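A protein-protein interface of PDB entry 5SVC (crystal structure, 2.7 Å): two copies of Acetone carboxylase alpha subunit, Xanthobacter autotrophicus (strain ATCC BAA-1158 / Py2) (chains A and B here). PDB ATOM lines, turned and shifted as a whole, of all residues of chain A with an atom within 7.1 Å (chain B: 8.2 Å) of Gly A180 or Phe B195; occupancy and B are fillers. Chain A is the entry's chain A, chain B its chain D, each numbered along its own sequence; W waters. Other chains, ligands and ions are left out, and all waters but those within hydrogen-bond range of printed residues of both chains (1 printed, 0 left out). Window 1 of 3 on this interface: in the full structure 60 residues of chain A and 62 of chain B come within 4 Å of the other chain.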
ATOM      1  N   CYS A 152      37.892  12.597   2.532  1.00  0.00           N
ATOM      2  CA  CYS A 152      36.803  12.095   1.706  1.00  0.00           C
ATOM      3  C   CYS A 152      37.049  10.703   1.174  1.00  0.00           C
ATOM      4  O   CYS A 152      36.118  10.119   0.608  1.00  0.00           O
ATOM      5  CB  CYS A 152      36.518  13.038   0.524  1.00  0.00           C
ATOM      6  SG  CYS A 152      35.315  14.235   1.042  1.00  0.00           S
ATOM      7  N   ILE A 177      31.233  11.734  -1.381  1.00  0.00           N
ATOM      8  CA  ILE A 177      30.956  13.081  -1.886  1.00  0.00           C
ATOM      9  C   ILE A 177      31.465  14.135  -0.916  1.00  0.00           C
ATOM     10  O   ILE A 177      32.033  15.147  -1.333  1.00  0.00           O
ATOM     11  CB  ILE A 177      29.457  13.307  -2.143  1.00  0.00           C
ATOM     12  CG1 ILE A 177      28.890  12.392  -3.216  1.00  0.00           C
ATOM     13  CG2 ILE A 177      29.251  14.741  -2.603  1.00  0.00           C
ATOM     14  CD1 ILE A 177      27.329  12.539  -3.356  1.00  0.00           C
ATOM     15  N   ASP A 178      31.234  13.953   0.381  1.00  0.00           N
ATOM     16  CA  ASP A 178      31.628  15.000   1.317  1.00  0.00           C
ATOM     17  C   ASP A 178      31.725  14.410   2.702  1.00  0.00           C
ATOM     18  O   ASP A 178      31.090  13.398   3.011  1.00  0.00           O
ATOM     19  CB  ASP A 178      30.665  16.196   1.340  1.00  0.00           C
ATOM     20  CG  ASP A 178      29.421  15.934   2.196  1.00  0.00           C
ATOM     21  OD1 ASP A 178      28.470  15.245   1.686  1.00  0.00           O
ATOM     22  OD2 ASP A 178      29.389  16.441   3.365  1.00  0.00           O
ATOM     23  N   THR A 179      32.522  15.072   3.532  1.00  0.00           N
ATOM     24  CA  THR A 179      32.762  14.630   4.893  1.00  0.00           C
ATOM     25  C   THR A 179      32.511  15.744   5.894  1.00  0.00           C
ATOM     26  O   THR A 179      33.078  15.739   6.999  1.00  0.00           O
ATOM     27  CB  THR A 179      34.183  14.132   5.006  1.00  0.00           C
ATOM     28  OG1 THR A 179      34.966  14.885   4.063  1.00  0.00           O
ATOM     29  CG2 THR A 179      34.203  12.629   4.660  1.00  0.00           C
ATOM     30  N   GLY A 180      31.666  16.698   5.514  1.00  0.00           N
ATOM     31  CA  GLY A 180      31.304  17.771   6.407  1.00  0.00           C
ATOM     32  C   GLY A 180      32.433  18.715   6.763  1.00  0.00           C
ATOM     33  O   GLY A 180      32.507  19.159   7.910  1.00  0.00           O
ATOM     34  N   ALA A 181      33.313  19.036   5.826  1.00  0.00           N
ATOM     35  CA  ALA A 181      34.203  20.177   6.047  1.00  0.00           C
ATOM     36  C   ALA A 181      33.446  21.501   5.877  1.00  0.00           C
ATOM     37  O   ALA A 181      32.278  21.535   5.481  1.00  0.00           O
ATOM     38  CB  ALA A 181      35.396  20.158   5.091  1.00  0.00           C
ATOM     39  N   VAL A 182      34.144  22.611   6.161  1.00  0.00           N
ATOM     40  CA  VAL A 182      33.546  23.939   5.984  1.00  0.00           C
ATOM     41  C   VAL A 182      33.094  24.125   4.544  1.00  0.00           C
ATOM     42  O   VAL A 182      31.946  24.499   4.271  1.00  0.00           O
ATOM     43  CB  VAL A 182      34.532  25.028   6.422  1.00  0.00           C
ATOM     44  CG1 VAL A 182      34.231  26.307   5.722  1.00  0.00           C
ATOM     45  CG2 VAL A 182      34.448  25.258   7.935  1.00  0.00           C
ATOM     46  N   GLY A 183      33.950  23.752   3.601  1.00  0.00           N
ATOM     47  CA  GLY A 183      33.577  23.788   2.217  1.00  0.00           C
ATOM     48  C   GLY A 183      32.580  22.708   1.865  1.00  0.00           C
ATOM     49  O   GLY A 183      32.679  21.538   2.276  1.00  0.00           O
ATOM     50  N   GLY A 185      31.641  20.252  -0.636  1.00  0.00           N
ATOM     51  CA  GLY A 185      32.308  19.537  -1.707  1.00  0.00           C
ATOM     52  C   GLY A 185      33.350  18.618  -1.095  1.00  0.00           C
ATOM     53  O   GLY A 185      33.552  18.598   0.121  1.00  0.00           O
ATOM     54  N   GLY A 196      37.883  21.763  10.972  1.00  0.00           N
ATOM     55  CA  GLY A 196      37.085  22.230   9.855  1.00  0.00           C
ATOM     56  C   GLY A 196      37.336  21.451   8.567  1.00  0.00           C
ATOM     57  O   GLY A 196      36.572  21.617   7.599  1.00  0.00           O
ATOM     58  N   ASP A 197      38.392  20.608   8.525  1.00  0.00           N
ATOM     59  CA  ASP A 197      38.708  19.830   7.335  1.00  0.00           C
ATOM     60  C   ASP A 197      37.856  18.548   7.199  1.00  0.00           C
ATOM     61  O   ASP A 197      38.084  17.794   6.242  1.00  0.00           O
ATOM     62  CB  ASP A 197      40.209  19.471   7.283  1.00  0.00           C
ATOM     63  CG  ASP A 197      40.710  19.174   5.816  1.00  0.00           C
ATOM     64  OD1 ASP A 197      40.021  19.537   4.853  1.00  0.00           O
ATOM     65  OD2 ASP A 197      41.779  18.569   5.606  1.00  0.00           O
ATOM     66  N   GLY A 198      36.872  18.308   8.069  1.00  0.00           N
ATOM     67  CA  GLY A 198      35.890  17.257   7.855  1.00  0.00           C
ATOM     68  C   GLY A 198      36.042  16.091   8.822  1.00  0.00           C
ATOM     69  O   GLY A 198      36.996  15.993   9.590  1.00  0.00           O
ATOM     70  N   TYR A 199      35.044  15.199   8.777  1.00  0.00           N
ATOM     71  CA  TYR A 199      34.877  14.078   9.712  1.00  0.00           C
ATOM     72  C   TYR A 199      36.081  13.145   9.680  1.00  0.00           C
ATOM     73  O   TYR A 199      36.300  12.449   8.686  1.00  0.00           O
ATOM     74  CB  TYR A 199      33.583  13.321   9.364  1.00  0.00           C
ATOM     75  CG  TYR A 199      33.099  12.332  10.409  1.00  0.00           C
ATOM     76  CD1 TYR A 199      32.743  12.745  11.683  1.00  0.00           C
ATOM     77  CD2 TYR A 199      32.973  10.981  10.113  1.00  0.00           C
ATOM     78  CE1 TYR A 199      32.290  11.833  12.637  1.00  0.00           C
ATOM     79  CE2 TYR A 199      32.516  10.060  11.061  1.00  0.00           C
ATOM     80  CZ  TYR A 199      32.175  10.481  12.326  1.00  0.00           C
ATOM     81  OH  TYR A 199      31.716   9.552  13.270  1.00  0.00           O
ATOM     82  N   GLN A 221      26.466   9.734  10.315  1.00  0.00           N
ATOM     83  CA  GLN A 221      25.649  10.209   9.193  1.00  0.00           C
ATOM     84  C   GLN A 221      25.272  11.691   9.310  1.00  0.00           C
ATOM     85  O   GLN A 221      25.037  12.351   8.285  1.00  0.00           O
ATOM     86  CB  GLN A 221      24.407   9.341   9.065  1.00  0.00           C
ATOM     87  CG  GLN A 221      24.713   7.950   8.571  1.00  0.00           C
ATOM     88  CD  GLN A 221      23.713   6.927   9.065  1.00  0.00           C
ATOM     89  OE1 GLN A 221      22.537   7.239   9.263  1.00  0.00           O
ATOM     90  NE2 GLN A 221      24.173   5.691   9.255  1.00  0.00           N
ATOM     91  N   ARG A 222      25.229  12.236  10.533  1.00  0.00           N
ATOM     92  CA  ARG A 222      24.899  13.636  10.750  1.00  0.00           C
ATOM     93  C   ARG A 222      26.126  14.545  10.756  1.00  0.00           C
ATOM     94  O   ARG A 222      25.986  15.762  10.928  1.00  0.00           O
ATOM     95  CB  ARG A 222      24.126  13.806  12.058  1.00  0.00           C
ATOM     96  CG  ARG A 222      24.993  13.721  13.327  1.00  0.00           C
ATOM     97  CD  ARG A 222      24.124  13.679  14.580  1.00  0.00           C
ATOM     98  NE  ARG A 222      23.092  12.648  14.444  1.00  0.00           N
ATOM     99  CZ  ARG A 222      22.150  12.391  15.338  1.00  0.00           C
ATOM    100  NH1 ARG A 222      21.279  11.432  15.100  1.00  0.00           N
ATOM    101  NH2 ARG A 222      22.073  13.092  16.461  1.00  0.00           N
ATOM    102  N   MET A 223      27.313  14.006  10.554  1.00  0.00           N
ATOM    103  CA  MET A 223      28.482  14.854  10.383  1.00  0.00           C
ATOM    104  C   MET A 223      28.695  15.271   8.938  1.00  0.00           C
ATOM    105  O   MET A 223      29.659  15.985   8.660  1.00  0.00           O
ATOM    106  CB  MET A 223      29.734  14.153  10.917  1.00  0.00           C
ATOM    107  CG  MET A 223      29.757  14.014  12.444  1.00  0.00           C
ATOM    108  SD  MET A 223      29.295  15.493  13.377  1.00  0.00           S
ATOM    109  CE  MET A 223      28.247  14.737  14.609  1.00  0.00           C
ATOM    110  N   VAL A 224      27.843  14.828   8.008  1.00  0.00           N
ATOM    111  CA  VAL A 224      28.010  15.128   6.589  1.00  0.00           C
ATOM    112  C   VAL A 224      26.729  15.661   5.962  1.00  0.00           C
ATOM    113  O   VAL A 224      25.643  15.613   6.537  1.00  0.00           O
ATOM    114  CB  VAL A 224      28.457  13.910   5.809  1.00  0.00           C
ATOM    115  CG1 VAL A 224      29.601  13.275   6.555  1.00  0.00           C
ATOM    116  CG2 VAL A 224      27.255  12.999   5.674  1.00  0.00           C
ATOM    117  N   ARG A 225      26.878  16.151   4.740  1.00  0.00           N
ATOM    118  CA  ARG A 225      25.717  16.640   4.025  1.00  0.00           C
ATOM    119  C   ARG A 225      25.017  15.494   3.331  1.00  0.00           C
ATOM    120  O   ARG A 225      23.838  15.232   3.595  1.00  0.00           O
ATOM    121  CB  ARG A 225      26.122  17.716   3.009  1.00  0.00           C
ATOM    122  CG  ARG A 225      26.570  19.058   3.609  1.00  0.00           C
ATOM    123  CD  ARG A 225      27.529  19.783   2.642  1.00  0.00           C
ATOM    124  NE  ARG A 225      28.706  20.175   3.403  1.00  0.00           N
ATOM    125  CZ  ARG A 225      28.895  21.395   3.896  1.00  0.00           C
ATOM    126  NH1 ARG A 225      29.986  21.651   4.622  1.00  0.00           N
ATOM    127  NH2 ARG A 225      28.006  22.361   3.641  1.00  0.00           N
ATOM    128  N   THR A 226      25.739  14.799   2.443  1.00  0.00           N
ATOM    129  CA  THR A 226      25.146  13.818   1.522  1.00  0.00           C
ATOM    130  C   THR A 226      25.024  12.437   2.186  1.00  0.00           C
ATOM    131  O   THR A 226      25.704  11.464   1.843  1.00  0.00           O
ATOM    132  CB  THR A 226      25.950  13.767   0.230  1.00  0.00           C
ATOM    133  OG1 THR A 226      27.331  13.517   0.528  1.00  0.00           O
ATOM    134  CG2 THR A 226      25.837  15.109  -0.479  1.00  0.00           C
ATOM    135  N   ILE A 450      19.390  18.637   1.771  1.00  0.00           N
ATOM    136  CA  ILE A 450      20.764  19.059   1.972  1.00  0.00           C
ATOM    137  C   ILE A 450      21.688  18.188   1.153  1.00  0.00           C
ATOM    138  O   ILE A 450      21.545  16.958   1.132  1.00  0.00           O
ATOM    139  CB  ILE A 450      21.092  18.962   3.469  1.00  0.00           C
ATOM    140  CG1 ILE A 450      20.133  19.829   4.260  1.00  0.00           C
ATOM    141  CG2 ILE A 450      22.555  19.294   3.749  1.00  0.00           C
ATOM    142  CD1 ILE A 450      20.580  20.003   5.636  1.00  0.00           C
ATOM    143  N   GLY B 180      38.233  21.657  19.004  1.00  0.00           N
ATOM    144  CA  GLY B 180      38.679  21.701  17.634  1.00  0.00           C
ATOM    145  C   GLY B 180      37.713  22.326  16.654  1.00  0.00           C
ATOM    146  O   GLY B 180      37.578  21.823  15.539  1.00  0.00           O
ATOM    147  N   ALA B 181      37.032  23.399  17.031  1.00  0.00           N
ATOM    148  CA  ALA B 181      36.300  24.175  16.027  1.00  0.00           C
ATOM    149  C   ALA B 181      37.277  24.990  15.165  1.00  0.00           C
ATOM    150  O   ALA B 181      38.486  24.968  15.364  1.00  0.00           O
ATOM    151  CB  ALA B 181      35.281  25.099  16.692  1.00  0.00           C
ATOM    152  N   VAL B 182      36.740  25.692  14.159  1.00  0.00           N
ATOM    153  CA  VAL B 182      37.563  26.585  13.336  1.00  0.00           C
ATOM    154  C   VAL B 182      38.194  27.662  14.206  1.00  0.00           C
ATOM    155  O   VAL B 182      39.368  28.009  14.041  1.00  0.00           O
ATOM    156  CB  VAL B 182      36.737  27.191  12.183  1.00  0.00           C
ATOM    157  CG1 VAL B 182      37.390  28.454  11.654  1.00  0.00           C
ATOM    158  CG2 VAL B 182      36.541  26.208  11.045  1.00  0.00           C
ATOM    159  N   GLY B 190      34.118  31.919  13.748  1.00  0.00           N
ATOM    160  CA  GLY B 190      34.849  31.463  12.583  1.00  0.00           C
ATOM    161  C   GLY B 190      33.969  30.587  11.724  1.00  0.00           C
ATOM    162  O   GLY B 190      33.670  30.922  10.578  1.00  0.00           O
ATOM    163  N   GLN B 191      33.525  29.477  12.288  1.00  0.00           N
ATOM    164  CA  GLN B 191      32.583  28.580  11.638  1.00  0.00           C
ATOM    165  C   GLN B 191      31.156  29.133  11.682  1.00  0.00           C
ATOM    166  O   GLN B 191      30.763  29.853  12.616  1.00  0.00           O
ATOM    167  CB  GLN B 191      32.623  27.216  12.322  1.00  0.00           C
ATOM    168  CG  GLN B 191      31.781  27.222  13.558  1.00  0.00           C
ATOM    169  CD  GLN B 191      32.534  27.623  14.830  1.00  0.00           C
ATOM    170  OE1 GLN B 191      33.355  28.560  14.855  1.00  0.00           O
ATOM    171  NE2 GLN B 191      32.239  26.898  15.912  1.00  0.00           N
ATOM    172  N   VAL B 192      30.355  28.733  10.691  1.00  0.00           N
ATOM    173  CA  VAL B 192      29.033  29.319  10.496  1.00  0.00           C
ATOM    174  C   VAL B 192      27.953  28.234  10.371  1.00  0.00           C
ATOM    175  O   VAL B 192      26.749  28.527  10.376  1.00  0.00           O
ATOM    176  CB  VAL B 192      29.088  30.281   9.297  1.00  0.00           C
ATOM    177  CG1 VAL B 192      28.157  29.898   8.205  1.00  0.00           C
ATOM    178  CG2 VAL B 192      28.824  31.672   9.746  1.00  0.00           C
ATOM    179  N   GLN B 193      28.371  26.963  10.338  1.00  0.00           N
ATOM    180  CA  GLN B 193      27.487  25.794  10.282  1.00  0.00           C
ATOM    181  C   GLN B 193      27.956  24.758  11.301  1.00  0.00           C
ATOM    182  O   GLN B 193      28.968  24.932  11.982  1.00  0.00           O
ATOM    183  CB  GLN B 193      27.474  25.150   8.879  1.00  0.00           C
ATOM    184  CG  GLN B 193      26.711  25.887   7.787  1.00  0.00           C
ATOM    185  CD  GLN B 193      26.687  25.132   6.462  1.00  0.00           C
ATOM    186  OE1 GLN B 193      27.703  24.665   6.011  1.00  0.00           O
ATOM    187  NE2 GLN B 193      25.535  25.086   5.805  1.00  0.00           N
ATOM    188  N   ARG B 194      27.242  23.636  11.378  1.00  0.00           N
ATOM    189  CA  ARG B 194      27.736  22.538  12.197  1.00  0.00           C
ATOM    190  C   ARG B 194      29.100  22.079  11.708  1.00  0.00           C
ATOM    191  O   ARG B 194      29.981  21.768  12.509  1.00  0.00           O
ATOM    192  CB  ARG B 194      26.742  21.384  12.192  1.00  0.00           C
ATOM    193  CG  ARG B 194      27.172  20.176  13.015  1.00  0.00           C
ATOM    194  CD  ARG B 194      26.317  18.948  12.682  1.00  0.00           C
ATOM    195  NE  ARG B 194      26.501  17.852  13.622  1.00  0.00           N
ATOM    196  CZ  ARG B 194      26.033  17.861  14.865  1.00  0.00           C
ATOM    197  NH1 ARG B 194      25.361  18.921  15.285  1.00  0.00           N
ATOM    198  NH2 ARG B 194      26.240  16.828  15.688  1.00  0.00           N
ATOM    199  N   PHE B 195      29.288  22.020  10.396  1.00  0.00           N
ATOM    200  CA  PHE B 195      30.542  21.576   9.779  1.00  0.00           C
ATOM    201  C   PHE B 195      31.671  22.569  10.039  1.00  0.00           C
ATOM    202  O   PHE B 195      31.803  23.566   9.336  1.00  0.00           O
ATOM    203  CB  PHE B 195      30.311  21.398   8.291  1.00  0.00           C
ATOM    204  CG  PHE B 195      29.003  20.772   7.989  1.00  0.00           C
ATOM    205  CD1 PHE B 195      28.761  19.455   8.361  1.00  0.00           C
ATOM    206  CD2 PHE B 195      28.006  21.495   7.350  1.00  0.00           C
ATOM    207  CE1 PHE B 195      27.526  18.850   8.104  1.00  0.00           C
ATOM    208  CE2 PHE B 195      26.771  20.919   7.082  1.00  0.00           C
ATOM    209  CZ  PHE B 195      26.529  19.587   7.461  1.00  0.00           C
ATOM    210  N   GLY B 196      32.516  22.276  11.024  1.00  0.00           N
ATOM    211  CA  GLY B 196      33.499  23.201  11.549  1.00  0.00           C
ATOM    212  C   GLY B 196      33.271  23.607  12.991  1.00  0.00           C
ATOM    213  O   GLY B 196      34.178  24.175  13.616  1.00  0.00           O
ATOM    214  N   ASP B 197      32.114  23.293  13.558  1.00  0.00           N
ATOM    215  CA  ASP B 197      31.802  23.707  14.919  1.00  0.00           C
ATOM    216  C   ASP B 197      32.422  22.801  16.007  1.00  0.00           C
ATOM    217  O   ASP B 197      32.165  23.026  17.202  1.00  0.00           O
ATOM    218  CB  ASP B 197      30.280  23.823  15.086  1.00  0.00           C
ATOM    219  CG  ASP B 197      29.901  24.703  16.272  1.00  0.00           C
ATOM    220  OD1 ASP B 197      30.829  25.395  16.755  1.00  0.00           O
ATOM    221  OD2 ASP B 197      28.715  24.714  16.711  1.00  0.00           O
ATOM    222  N   GLY B 198      33.258  21.834  15.650  1.00  0.00           N
ATOM    223  CA  GLY B 198      34.043  21.117  16.635  1.00  0.00           C
ATOM    224  C   GLY B 198      33.565  19.685  16.826  1.00  0.00           C
ATOM    225  O   GLY B 198      32.487  19.288  16.389  1.00  0.00           O
ATOM    226  N   PRO B 306      33.742  32.255   6.102  1.00  0.00           N
ATOM    227  CA  PRO B 306      33.986  31.816   4.716  1.00  0.00           C
ATOM    228  C   PRO B 306      32.761  31.862   3.837  1.00  0.00           C
ATOM    229  O   PRO B 306      32.900  31.927   2.603  1.00  0.00           O
ATOM    230  CB  PRO B 306      34.494  30.376   4.881  1.00  0.00           C
ATOM    231  CG  PRO B 306      34.044  29.946   6.220  1.00  0.00           C
ATOM    232  CD  PRO B 306      33.854  31.159   7.082  1.00  0.00           C
ATOM    233  N   SER B 307      31.576  31.850   4.435  1.00  0.00           N
ATOM    234  CA  SER B 307      30.320  31.704   3.719  1.00  0.00           C
ATOM    235  C   SER B 307      29.705  33.085   3.525  1.00  0.00           C
ATOM    236  O   SER B 307      29.405  33.771   4.503  1.00  0.00           O
ATOM    237  CB  SER B 307      29.375  30.789   4.498  1.00  0.00           C
ATOM    238  OG  SER B 307      30.039  29.600   4.906  1.00  0.00           O
ATOM    239  N   TRP B 342      23.017  31.701  10.510  1.00  0.00           N
ATOM    240  CA  TRP B 342      24.343  31.198  10.169  1.00  0.00           C
ATOM    241  C   TRP B 342      25.346  31.902  11.082  1.00  0.00           C
ATOM    242  O   TRP B 342      26.005  32.876  10.729  1.00  0.00           O
ATOM    243  CB  TRP B 342      24.639  31.409   8.688  1.00  0.00           C
ATOM    244  CG  TRP B 342      23.552  30.886   7.767  1.00  0.00           C
ATOM    245  CD1 TRP B 342      22.624  31.622   7.044  1.00  0.00           C
ATOM    246  CD2 TRP B 342      23.283  29.522   7.467  1.00  0.00           C
ATOM    247  NE1 TRP B 342      21.812  30.792   6.330  1.00  0.00           N
ATOM    248  CE2 TRP B 342      22.197  29.497   6.567  1.00  0.00           C
ATOM    249  CE3 TRP B 342      23.855  28.312   7.868  1.00  0.00           C
ATOM    250  CZ2 TRP B 342      21.686  28.308   6.064  1.00  0.00           C
ATOM    251  CZ3 TRP B 342      23.346  27.143   7.372  1.00  0.00           C
ATOM    252  CH2 TRP B 342      22.261  27.144   6.490  1.00  0.00           C
ATOM    253  N   ASP B 392      16.742  22.621  11.554  1.00  0.00           N
ATOM    254  CA  ASP B 392      17.802  22.428  10.574  1.00  0.00           C
ATOM    255  C   ASP B 392      19.026  21.803  11.233  1.00  0.00           C
ATOM    256  O   ASP B 392      19.472  22.267  12.286  1.00  0.00           O
ATOM    257  CB  ASP B 392      18.188  23.742   9.918  1.00  0.00           C
ATOM    258  CG  ASP B 392      18.895  23.522   8.621  1.00  0.00           C
ATOM    259  OD1 ASP B 392      18.201  23.379   7.588  1.00  0.00           O
ATOM    260  OD2 ASP B 392      20.141  23.427   8.643  1.00  0.00           O
ATOM    261  N   ARG B 393      19.593  20.780  10.592  1.00  0.00           N
ATOM    262  CA  ARG B 393      20.693  20.019  11.173  1.00  0.00           C
ATOM    263  C   ARG B 393      22.072  20.525  10.733  1.00  0.00           C
ATOM    264  O   ARG B 393      23.085  19.939  11.151  1.00  0.00           O
ATOM    265  CB  ARG B 393      20.532  18.530  10.832  1.00  0.00           C
ATOM    266  CG  ARG B 393      20.784  18.242   9.356  1.00  0.00           C
ATOM    267  CD  ARG B 393      20.455  16.838   8.971  1.00  0.00           C
ATOM    268  NE  ARG B 393      20.655  16.577   7.547  1.00  0.00           N
ATOM    269  CZ  ARG B 393      21.833  16.265   7.012  1.00  0.00           C
ATOM    270  NH1 ARG B 393      22.915  16.204   7.779  1.00  0.00           N
ATOM    271  NH2 ARG B 393      21.926  16.025   5.710  1.00  0.00           N
ATOM    272  N   ARG B 394      22.139  21.608   9.927  1.00  0.00           N
ATOM    273  CA  ARG B 394      23.406  22.291   9.639  1.00  0.00           C
ATOM    274  C   ARG B 394      23.812  23.303  10.716  1.00  0.00           C
ATOM    275  O   ARG B 394      24.989  23.667  10.788  1.00  0.00           O
ATOM    276  CB  ARG B 394      23.343  22.999   8.283  1.00  0.00           C
ATOM    277  CG  ARG B 394      23.346  22.040   7.076  1.00  0.00           C
ATOM    278  CD  ARG B 394      22.957  22.735   5.779  1.00  0.00           C
ATOM    279  NE  ARG B 394      21.577  23.212   5.836  1.00  0.00           N
ATOM    280  CZ  ARG B 394      21.088  24.166   5.056  1.00  0.00           C
ATOM    281  NH1 ARG B 394      21.883  24.750   4.165  1.00  0.00           N
ATOM    282  NH2 ARG B 394      19.818  24.553   5.186  1.00  0.00           N
ATOM    283  N   VAL B 395      22.881  23.712  11.578  1.00  0.00           N
ATOM    284  CA  VAL B 395      23.036  24.692  12.659  1.00  0.00           C
ATOM    285  C   VAL B 395      24.300  24.528  13.521  1.00  0.00           C
ATOM    286  O   VAL B 395      24.774  23.402  13.757  1.00  0.00           O
ATOM    287  CB  VAL B 395      21.750  24.604  13.510  1.00  0.00           C
ATOM    288  CG1 VAL B 395      21.901  25.250  14.850  1.00  0.00           C
ATOM    289  CG2 VAL B 395      20.582  25.200  12.753  1.00  0.00           C
ATOM    290  N   ALA B 396      24.832  25.643  14.042  1.00  0.00           N
ATOM    291  CA  ALA B 396      26.012  25.613  14.894  1.00  0.00           C
ATOM    292  C   ALA B 396      25.727  26.176  16.294  1.00  0.00           C
ATOM    293  O   ALA B 396      24.866  27.032  16.483  1.00  0.00           O
ATOM    294  CB  ALA B 396      27.168  26.359  14.246  1.00  0.00           C
HETATM  295  O   HOH W   1      26.461  23.971   2.624  1.00  0.00           O
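The backbone carbonyl oxygen (O) of Arg A222 lies within hydrogen-bond range of the guanidinium group (NE) of Arg B194.
NE of Arg B194 lies within hydrogen-bond range of SD of Met A223 (3.7 Å).
The guanidinium group (NH1) of Arg B393 sits at hydrogen-bond distance from the backbone carbonyl oxygen (O) of Val A224 (3.1 Å).
NH2 of Arg A225 is in hydrogen-bond range of OE1 of Gln B193.
The guanidinium group of Arg B393 is in hydrogen-bond range of the backbone carbonyl oxygen of Arg A225, at 3.0 Å.
N of Gly A180 lies within hydrogen-bond range of OD2 of Asp A178 (3.1 Å).
The guanidinium group (NH1) of Arg A225 lies within hydrogen-bond range of the backbone carbonyl oxygen (O) of Ala A181 (2.5 Å).
N of Val A182 sits at hydrogen-bond distance from O of Gly A196, 3.0 Å away.
N of Val B182 sits at hydrogen-bond distance from O of Gly B196 (3.0 Å).
O of Val B395 lies close to N of Arg B194.
The side-chain carboxylate (OD1) of Asp B392 lies within salt-bridge range of the guanidinium group (NH2) of Arg B394 (3.1 Å).
Among the printed residues, pairs that only touch across the chains: Gly A180 with Phe B195 (3.2 Å), Ile A450 with Arg B394 (3.4 Å), Arg A225 with Phe B195 (3.4 Å), Ala A181 with Phe B195 (3.4 Å), Val A182 with Phe B195 (3.4 Å), Met A223 with Phe B195 (3.6 Å), Val A182 with Pro B306 (3.7 Å), Ile A450 with Arg B393 (3.8 Å), Val A182 with Val B182 (3.9 Å) and Val A224 with Phe B195 (3.9 Å).
Of chain B, only Phe B195 comes within 4 Å of Gly A180.
Ala A181 touches just one residue of chain B: Phe B195 (3.4 Å).
Of the printed residues of chain B, Arg A222 touches Arg B194 (3.4 Å).
Printed residues of chain A within 4 Å of Val B182: Val A182 (3.9 Å).
Phe B195 touches six residues of chain A.
The nearest residue of chain A that does not touch Phe B195 is Arg A222 (4.5 Å).
The nearest printed residue of chain A that does not touch Gln B193 is Val A182 (4.6 Å).
Printed residues of chain B that touch a printed residue of chain A: Val B182, Gln B193, Arg B194, Phe B195, Pro B306, Arg B393 and Arg B394.
Hydrophobic or aromatic side chains of chain B within 4 Å of the printed part of chain A: Val B182, Phe B195 and Pro B306.
Printed residues of chain A that touch a printed residue of chain B: Gly A180, Ala A181, Val A182, Arg A222, Met A223, Val A224, Arg A225 and Ile A450.
Hydrophobic or aromatic side chains of chain A that line the printed part of chain B: Val A182, Met A223 and Ile A450.
Val A182 touches its own counterpart, Val B182.
6 positions are printed for both chains.
Of the 15 pairs that touch across the chains among the printed residues, 1 has its exchanged pair printed and touching as well.
Water W1 bridges the guanidinium group of Arg A225 and the side-chain amide nitrogen of Gln B193.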
